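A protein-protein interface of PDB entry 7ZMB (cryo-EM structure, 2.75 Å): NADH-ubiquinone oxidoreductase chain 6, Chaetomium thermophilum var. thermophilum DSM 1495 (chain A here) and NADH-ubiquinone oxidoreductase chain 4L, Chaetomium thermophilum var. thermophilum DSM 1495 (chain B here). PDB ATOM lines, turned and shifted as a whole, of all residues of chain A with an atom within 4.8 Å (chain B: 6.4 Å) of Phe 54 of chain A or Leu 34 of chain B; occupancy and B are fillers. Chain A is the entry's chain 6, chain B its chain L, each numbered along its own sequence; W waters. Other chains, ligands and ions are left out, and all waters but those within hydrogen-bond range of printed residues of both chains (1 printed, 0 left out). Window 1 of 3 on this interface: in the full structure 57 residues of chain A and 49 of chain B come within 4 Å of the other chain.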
ATOM      1  N   LEU A  50     -17.343  18.804  32.801  1.00  0.00           N
ATOM      2  CA  LEU A  50     -16.617  19.419  31.701  1.00  0.00           C
ATOM      3  C   LEU A  50     -17.082  18.867  30.361  1.00  0.00           C
ATOM      4  O   LEU A  50     -17.332  19.626  29.422  1.00  0.00           O
ATOM      5  CB  LEU A  50     -15.115  19.211  31.894  1.00  0.00           C
ATOM      6  CG  LEU A  50     -14.168  19.741  30.822  1.00  0.00           C
ATOM      7  CD1 LEU A  50     -14.017  21.249  30.920  1.00  0.00           C
ATOM      8  CD2 LEU A  50     -12.839  19.069  30.977  1.00  0.00           C
ATOM      9  N   ILE A  51     -17.211  17.542  30.254  1.00  0.00           N
ATOM     10  CA  ILE A  51     -17.673  16.959  29.002  1.00  0.00           C
ATOM     11  C   ILE A  51     -19.148  17.265  28.785  1.00  0.00           C
ATOM     12  O   ILE A  51     -19.591  17.442  27.646  1.00  0.00           O
ATOM     13  CB  ILE A  51     -17.371  15.443  28.947  1.00  0.00           C
ATOM     14  CG1 ILE A  51     -17.802  14.847  27.606  1.00  0.00           C
ATOM     15  CG2 ILE A  51     -18.020  14.698  30.075  1.00  0.00           C
ATOM     16  CD1 ILE A  51     -17.061  15.419  26.409  1.00  0.00           C
ATOM     17  N   GLY A  52     -19.926  17.355  29.861  1.00  0.00           N
ATOM     18  CA  GLY A  52     -21.301  17.799  29.721  1.00  0.00           C
ATOM     19  C   GLY A  52     -21.394  19.211  29.183  1.00  0.00           C
ATOM     20  O   GLY A  52     -22.244  19.508  28.344  1.00  0.00           O
ATOM     21  N   LEU A  53     -20.481  20.105  29.586  1.00  0.00           N
ATOM     22  CA  LEU A  53     -20.490  21.521  29.129  1.00  0.00           C
ATOM     23  C   LEU A  53     -20.260  21.568  27.623  1.00  0.00           C
ATOM     24  O   LEU A  53     -21.032  22.232  26.939  1.00  0.00           O
ATOM     25  CB  LEU A  53     -19.385  22.272  29.885  1.00  0.00           C
ATOM     26  CG  LEU A  53     -18.921  23.610  29.317  1.00  0.00           C
ATOM     27  CD1 LEU A  53     -20.001  24.668  29.440  1.00  0.00           C
ATOM     28  CD2 LEU A  53     -17.661  24.066  30.028  1.00  0.00           C
ATOM     29  N   PHE A  54     -19.254  20.852  27.139  1.00  0.00           N
ATOM     30  CA  PHE A  54     -18.940  20.816  25.691  1.00  0.00           C
ATOM     31  C   PHE A  54     -20.106  20.184  24.917  1.00  0.00           C
ATOM     32  O   PHE A  54     -20.341  20.605  23.794  1.00  0.00           O
ATOM     33  CB  PHE A  54     -17.605  20.108  25.458  1.00  0.00           C
ATOM     34  CG  PHE A  54     -16.366  20.915  25.731  1.00  0.00           C
ATOM     35  CD1 PHE A  54     -15.851  21.768  24.769  1.00  0.00           C
ATOM     36  CD2 PHE A  54     -15.693  20.795  26.934  1.00  0.00           C
ATOM     37  CE1 PHE A  54     -14.705  22.502  25.018  1.00  0.00           C
ATOM     38  CE2 PHE A  54     -14.545  21.527  27.180  1.00  0.00           C
ATOM     39  CZ  PHE A  54     -14.058  22.383  26.225  1.00  0.00           C
ATOM     40  N   ALA A  55     -20.800  19.211  25.510  1.00  0.00           N
ATOM     41  CA  ALA A  55     -21.922  18.547  24.813  1.00  0.00           C
ATOM     42  C   ALA A  55     -23.085  19.525  24.646  1.00  0.00           C
ATOM     43  O   ALA A  55     -23.651  19.571  23.559  1.00  0.00           O
ATOM     44  CB  ALA A  55     -22.348  17.313  25.558  1.00  0.00           C
ATOM     45  N   TYR A  56     -23.364  20.322  25.671  1.00  0.00           N
ATOM     46  CA  TYR A  56     -24.464  21.304  25.566  1.00  0.00           C
ATOM     47  C   TYR A  56     -24.093  22.389  24.564  1.00  0.00           C
ATOM     48  O   TYR A  56     -24.981  22.821  23.814  1.00  0.00           O
ATOM     49  CB  TYR A  56     -24.916  21.853  26.917  1.00  0.00           C
ATOM     50  CG  TYR A  56     -25.279  20.824  27.954  1.00  0.00           C
ATOM     51  CD1 TYR A  56     -26.108  19.760  27.646  1.00  0.00           C
ATOM     52  CD2 TYR A  56     -24.809  20.933  29.250  1.00  0.00           C
ATOM     53  CE1 TYR A  56     -26.450  18.818  28.601  1.00  0.00           C
ATOM     54  CE2 TYR A  56     -25.143  20.000  30.216  1.00  0.00           C
ATOM     55  CZ  TYR A  56     -25.965  18.941  29.889  1.00  0.00           C
ATOM     56  OH  TYR A  56     -26.290  18.018  30.838  1.00  0.00           O
ATOM     57  N   VAL A  57     -22.837  22.828  24.576  1.00  0.00           N
ATOM     58  CA  VAL A  57     -22.373  23.868  23.614  1.00  0.00           C
ATOM     59  C   VAL A  57     -22.448  23.284  22.205  1.00  0.00           C
ATOM     60  O   VAL A  57     -22.902  23.980  21.313  1.00  0.00           O
ATOM     61  CB  VAL A  57     -20.985  24.412  24.011  1.00  0.00           C
ATOM     62  CG1 VAL A  57     -20.378  25.270  22.910  1.00  0.00           C
ATOM     63  CG2 VAL A  57     -21.043  25.187  25.316  1.00  0.00           C
ATOM     64  N   SER A  58     -22.039  22.032  22.039  1.00  0.00           N
ATOM     65  CA  SER A  58     -22.078  21.328  20.732  1.00  0.00           C
ATOM     66  C   SER A  58     -23.510  21.086  20.248  1.00  0.00           C
ATOM     67  O   SER A  58     -23.748  21.242  19.054  1.00  0.00           O
ATOM     68  CB  SER A  58     -21.292  20.057  20.809  1.00  0.00           C
ATOM     69  OG  SER A  58     -21.791  19.095  19.897  1.00  0.00           O
ATOM     70  N   TYR A  73     -16.454  19.504  17.437  1.00  0.00           N
ATOM     71  CA  TYR A  73     -16.186  19.885  18.840  1.00  0.00           C
ATOM     72  C   TYR A  73     -16.407  18.678  19.742  1.00  0.00           C
ATOM     73  O   TYR A  73     -15.535  18.369  20.544  1.00  0.00           O
ATOM     74  CB  TYR A  73     -17.166  20.974  19.279  1.00  0.00           C
ATOM     75  CG  TYR A  73     -16.538  22.229  19.823  1.00  0.00           C
ATOM     76  CD1 TYR A  73     -15.941  22.242  21.069  1.00  0.00           C
ATOM     77  CD2 TYR A  73     -16.552  23.407  19.099  1.00  0.00           C
ATOM     78  CE1 TYR A  73     -15.358  23.388  21.578  1.00  0.00           C
ATOM     79  CE2 TYR A  73     -15.976  24.563  19.593  1.00  0.00           C
ATOM     80  CZ  TYR A  73     -15.379  24.555  20.840  1.00  0.00           C
ATOM     81  OH  TYR A  73     -14.814  25.684  21.349  1.00  0.00           O
ATOM     82  N   LEU A  74     -17.531  18.000  19.584  1.00  0.00           N
ATOM     83  CA  LEU A  74     -17.842  16.848  20.469  1.00  0.00           C
ATOM     84  C   LEU A  74     -16.837  15.716  20.201  1.00  0.00           C
ATOM     85  O   LEU A  74     -16.281  15.223  21.169  1.00  0.00           O
ATOM     86  CB  LEU A  74     -19.290  16.423  20.186  1.00  0.00           C
ATOM     87  CG  LEU A  74     -19.976  15.536  21.218  1.00  0.00           C
ATOM     88  CD1 LEU A  74     -20.091  16.251  22.553  1.00  0.00           C
ATOM     89  CD2 LEU A  74     -21.348  15.120  20.714  1.00  0.00           C
ATOM     90  N   TYR A  77     -13.395  16.961  21.734  1.00  0.00           N
ATOM     91  CA  TYR A  77     -13.342  17.241  23.188  1.00  0.00           C
ATOM     92  C   TYR A  77     -13.765  16.026  24.010  1.00  0.00           C
ATOM     93  O   TYR A  77     -13.550  16.075  25.216  1.00  0.00           O
ATOM     94  CB  TYR A  77     -13.971  18.591  23.527  1.00  0.00           C
ATOM     95  CG  TYR A  77     -13.079  19.726  23.111  1.00  0.00           C
ATOM     96  CD1 TYR A  77     -11.929  20.011  23.818  1.00  0.00           C
ATOM     97  CD2 TYR A  77     -13.339  20.457  21.968  1.00  0.00           C
ATOM     98  CE1 TYR A  77     -11.074  21.020  23.418  1.00  0.00           C
ATOM     99  CE2 TYR A  77     -12.503  21.483  21.564  1.00  0.00           C
ATOM    100  CZ  TYR A  77     -11.367  21.768  22.295  1.00  0.00           C
ATOM    101  OH  TYR A  77     -10.529  22.771  21.910  1.00  0.00           O
ATOM    102  N   LEU B   7     -19.901  32.158  30.092  1.00  0.00           N
ATOM    103  CA  LEU B   7     -18.893  31.107  30.030  1.00  0.00           C
ATOM    104  C   LEU B   7     -17.492  31.669  30.211  1.00  0.00           C
ATOM    105  O   LEU B   7     -16.663  31.055  30.891  1.00  0.00           O
ATOM    106  CB  LEU B   7     -18.990  30.348  28.710  1.00  0.00           C
ATOM    107  CG  LEU B   7     -20.079  29.292  28.539  1.00  0.00           C
ATOM    108  CD1 LEU B   7     -19.744  28.420  27.353  1.00  0.00           C
ATOM    109  CD2 LEU B   7     -20.257  28.459  29.791  1.00  0.00           C
ATOM    110  N   ILE B  29      -8.702  27.364  31.328  1.00  0.00           N
ATOM    111  CA  ILE B  29      -8.282  27.934  30.053  1.00  0.00           C
ATOM    112  C   ILE B  29      -9.112  27.346  28.925  1.00  0.00           C
ATOM    113  O   ILE B  29      -9.579  28.065  28.035  1.00  0.00           O
ATOM    114  CB  ILE B  29      -6.778  27.701  29.836  1.00  0.00           C
ATOM    115  CG1 ILE B  29      -5.962  28.726  30.623  1.00  0.00           C
ATOM    116  CG2 ILE B  29      -6.435  27.750  28.361  1.00  0.00           C
ATOM    117  CD1 ILE B  29      -4.589  28.233  31.020  1.00  0.00           C
ATOM    118  N   GLU B  30      -9.337  26.033  28.980  1.00  0.00           N
ATOM    119  CA  GLU B  30     -10.133  25.323  27.957  1.00  0.00           C
ATOM    120  C   GLU B  30     -11.556  25.884  27.913  1.00  0.00           C
ATOM    121  O   GLU B  30     -12.140  25.887  26.832  1.00  0.00           O
ATOM    122  CB  GLU B  30     -10.168  23.841  28.307  1.00  0.00           C
ATOM    123  CG  GLU B  30      -8.822  23.152  28.334  1.00  0.00           C
ATOM    124  CD  GLU B  30      -8.925  21.668  28.643  1.00  0.00           C
ATOM    125  OE1 GLU B  30     -10.061  21.147  28.653  1.00  0.00           O
ATOM    126  OE2 GLU B  30      -7.875  21.038  28.883  1.00  0.00           O
ATOM    127  N   ILE B  31     -12.090  26.333  29.045  1.00  0.00           N
ATOM    128  CA  ILE B  31     -13.425  26.909  29.056  1.00  0.00           C
ATOM    129  C   ILE B  31     -13.419  28.291  28.416  1.00  0.00           C
ATOM    130  O   ILE B  31     -14.317  28.630  27.641  1.00  0.00           O
ATOM    131  CB  ILE B  31     -13.976  26.940  30.490  1.00  0.00           C
ATOM    132  CG1 ILE B  31     -14.216  25.518  30.984  1.00  0.00           C
ATOM    133  CG2 ILE B  31     -15.254  27.748  30.556  1.00  0.00           C
ATOM    134  CD1 ILE B  31     -14.646  25.447  32.435  1.00  0.00           C
ATOM    135  N   MET B  32     -12.416  29.105  28.717  1.00  0.00           N
ATOM    136  CA  MET B  32     -12.367  30.487  28.177  1.00  0.00           C
ATOM    137  C   MET B  32     -12.287  30.424  26.651  1.00  0.00           C
ATOM    138  O   MET B  32     -13.054  31.141  25.993  1.00  0.00           O
ATOM    139  CB  MET B  32     -11.192  31.277  28.752  1.00  0.00           C
ATOM    140  CG  MET B  32     -11.415  31.709  30.170  1.00  0.00           C
ATOM    141  SD  MET B  32     -10.052  32.689  30.810  1.00  0.00           S
ATOM    142  CE  MET B  32      -8.884  31.404  31.248  1.00  0.00           C
ATOM    143  N   LEU B  33     -11.382  29.602  26.123  1.00  0.00           N
ATOM    144  CA  LEU B  33     -11.215  29.460  24.659  1.00  0.00           C
ATOM    145  C   LEU B  33     -12.529  28.989  24.052  1.00  0.00           C
ATOM    146  O   LEU B  33     -12.868  29.472  22.970  1.00  0.00           O
ATOM    147  CB  LEU B  33     -10.103  28.444  24.394  1.00  0.00           C
ATOM    148  CG  LEU B  33      -8.716  28.850  24.895  1.00  0.00           C
ATOM    149  CD1 LEU B  33      -7.718  27.718  24.742  1.00  0.00           C
ATOM    150  CD2 LEU B  33      -8.222  30.093  24.183  1.00  0.00           C
ATOM    151  N   LEU B  34     -13.235  28.094  24.738  1.00  0.00           N
ATOM    152  CA  LEU B  34     -14.524  27.559  24.240  1.00  0.00           C
ATOM    153  C   LEU B  34     -15.509  28.706  24.067  1.00  0.00           C
ATOM    154  O   LEU B  34     -16.142  28.762  23.001  1.00  0.00           O
ATOM    155  CB  LEU B  34     -15.052  26.554  25.261  1.00  0.00           C
ATOM    156  CG  LEU B  34     -16.563  26.323  25.251  1.00  0.00           C
ATOM    157  CD1 LEU B  34     -16.965  25.390  24.124  1.00  0.00           C
ATOM    158  CD2 LEU B  34     -17.032  25.765  26.583  1.00  0.00           C
ATOM    159  N   SER B  35     -15.633  29.567  25.077  1.00  0.00           N
ATOM    160  CA  SER B  35     -16.581  30.710  25.037  1.00  0.00           C
ATOM    161  C   SER B  35     -16.219  31.666  23.899  1.00  0.00           C
ATOM    162  O   SER B  35     -17.143  32.195  23.269  1.00  0.00           O
ATOM    163  CB  SER B  35     -16.557  31.426  26.353  1.00  0.00           C
ATOM    164  OG  SER B  35     -15.485  32.350  26.411  1.00  0.00           O
ATOM    165  N   ILE B  36     -14.922  31.921  23.695  1.00  0.00           N
ATOM    166  CA  ILE B  36     -14.462  32.828  22.601  1.00  0.00           C
ATOM    167  C   ILE B  36     -14.800  32.189  21.261  1.00  0.00           C
ATOM    168  O   ILE B  36     -15.344  32.893  20.416  1.00  0.00           O
ATOM    169  CB  ILE B  36     -12.957  33.171  22.731  1.00  0.00           C
ATOM    170  CG1 ILE B  36     -12.617  33.786  24.092  1.00  0.00           C
ATOM    171  CG2 ILE B  36     -12.473  34.047  21.591  1.00  0.00           C
ATOM    172  CD1 ILE B  36     -13.526  34.917  24.503  1.00  0.00           C
ATOM    173  N   THR B  37     -14.542  30.892  21.111  1.00  0.00           N
ATOM    174  CA  THR B  37     -14.867  30.164  19.859  1.00  0.00           C
ATOM    175  C   THR B  37     -16.373  30.266  19.608  1.00  0.00           C
ATOM    176  O   THR B  37     -16.759  30.476  18.459  1.00  0.00           O
ATOM    177  CB  THR B  37     -14.402  28.710  19.948  1.00  0.00           C
ATOM    178  OG1 THR B  37     -13.004  28.702  20.227  1.00  0.00           O
ATOM    179  CG2 THR B  37     -14.678  27.909  18.696  1.00  0.00           C
ATOM    180  N   PHE B  38     -17.166  30.156  20.670  1.00  0.00           N
ATOM    181  CA  PHE B  38     -18.641  30.212  20.568  1.00  0.00           C
ATOM    182  C   PHE B  38     -19.044  31.602  20.077  1.00  0.00           C
ATOM    183  O   PHE B  38     -19.900  31.691  19.193  1.00  0.00           O
ATOM    184  CB  PHE B  38     -19.229  29.857  21.939  1.00  0.00           C
ATOM    185  CG  PHE B  38     -20.637  29.327  21.956  1.00  0.00           C
ATOM    186  CD1 PHE B  38     -21.238  28.848  20.804  1.00  0.00           C
ATOM    187  CD2 PHE B  38     -21.353  29.287  23.140  1.00  0.00           C
ATOM    188  CE1 PHE B  38     -22.532  28.358  20.837  1.00  0.00           C
ATOM    189  CE2 PHE B  38     -22.646  28.791  23.173  1.00  0.00           C
ATOM    190  CZ  PHE B  38     -23.232  28.328  22.020  1.00  0.00           C
ATOM    191  N   LEU B  39     -18.425  32.645  20.620  1.00  0.00           N
ATOM    192  CA  LEU B  39     -18.731  34.016  20.147  1.00  0.00           C
ATOM    193  C   LEU B  39     -18.387  34.120  18.664  1.00  0.00           C
ATOM    194  O   LEU B  39     -19.180  34.709  17.927  1.00  0.00           O
ATOM    195  CB  LEU B  39     -17.975  35.055  20.975  1.00  0.00           C
ATOM    196  CG  LEU B  39     -18.145  36.488  20.486  1.00  0.00           C
ATOM    197  CD1 LEU B  39     -19.612  36.879  20.500  1.00  0.00           C
ATOM    198  CD2 LEU B  39     -17.305  37.447  21.307  1.00  0.00           C
ATOM    199  N   ILE B  59      -8.841  27.521  16.381  1.00  0.00           N
ATOM    200  CA  ILE B  59      -8.672  27.772  17.843  1.00  0.00           C
ATOM    201  C   ILE B  59      -8.866  26.442  18.561  1.00  0.00           C
ATOM    202  O   ILE B  59      -8.217  26.245  19.588  1.00  0.00           O
ATOM    203  CB  ILE B  59      -9.640  28.851  18.359  1.00  0.00           C
ATOM    204  CG1 ILE B  59      -9.377  30.217  17.725  1.00  0.00           C
ATOM    205  CG2 ILE B  59      -9.641  28.918  19.877  1.00  0.00           C
ATOM    206  CD1 ILE B  59     -10.566  31.136  17.786  1.00  0.00           C
HETATM  207  O   HOH W   1     -11.908  25.787  21.355  1.00  0.00           O
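The backbone carbonyl oxygen (O) of Leu 33 of chain B is in hydrogen-bond range of the side-chain hydroxyl (OG1) of Thr 37 of chain B.
Among the printed residues, pairs that only touch across the chains: Tyr 73 of chain A with Thr 37 of chain B (3.4 Å), Tyr 73 of chain A with Leu 34 of chain B (3.5 Å), Val 57 of chain A with Leu 34 of chain B (3.6 Å), Phe 54 of chain A with Leu 34 of chain B (3.8 Å), Leu 53 of chain A with Leu 7 of chain B (3.8 Å), Leu 53 of chain A with Ile 31 of chain B (3.9 Å) and Leu 53 of chain A with Leu 34 of chain B (3.9 Å).
Printed residues of chain B within 4 Å of Phe 54 of chain A: Leu 34.
Of the printed residues of chain A, Thr 37 of chain B touches Tyr 73 (3.4 Å).
Printed residues of chain A within 4 Å of Leu 7 of chain B: Leu 53 (3.8 Å).
Of the printed residues of chain B, Tyr 73 of chain A touches Leu 34 (3.5 Å) and Thr 37 (3.4 Å).
Of the printed residues of chain A, Ile 31 of chain B touches Leu 53 (3.9 Å).
Printed residues of chain B within 4 Å of Val 57 of chain A: Leu 34 (3.6 Å).
Phe 38 of chain B touches none of the printed residues of chain A.
Gly 52 of chain A touches none of the printed residues of chain B.
Printed residues of chain A that touch a printed residue of chain B: Leu 53, Phe 54, Val 57 and Tyr 73.
Among the printed residues, no Asp or Glu carboxylate lies within 4 Å of a Lys or Arg side-chain nitrogen of the other chain.
Water W1 lies within hydrogen-bond range of OH of Tyr 73 of chain A (2.9 Å), OG1 of Thr 37 of chain B (3.3 Å) and OH of Tyr 77 of chain A (3.4 Å).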
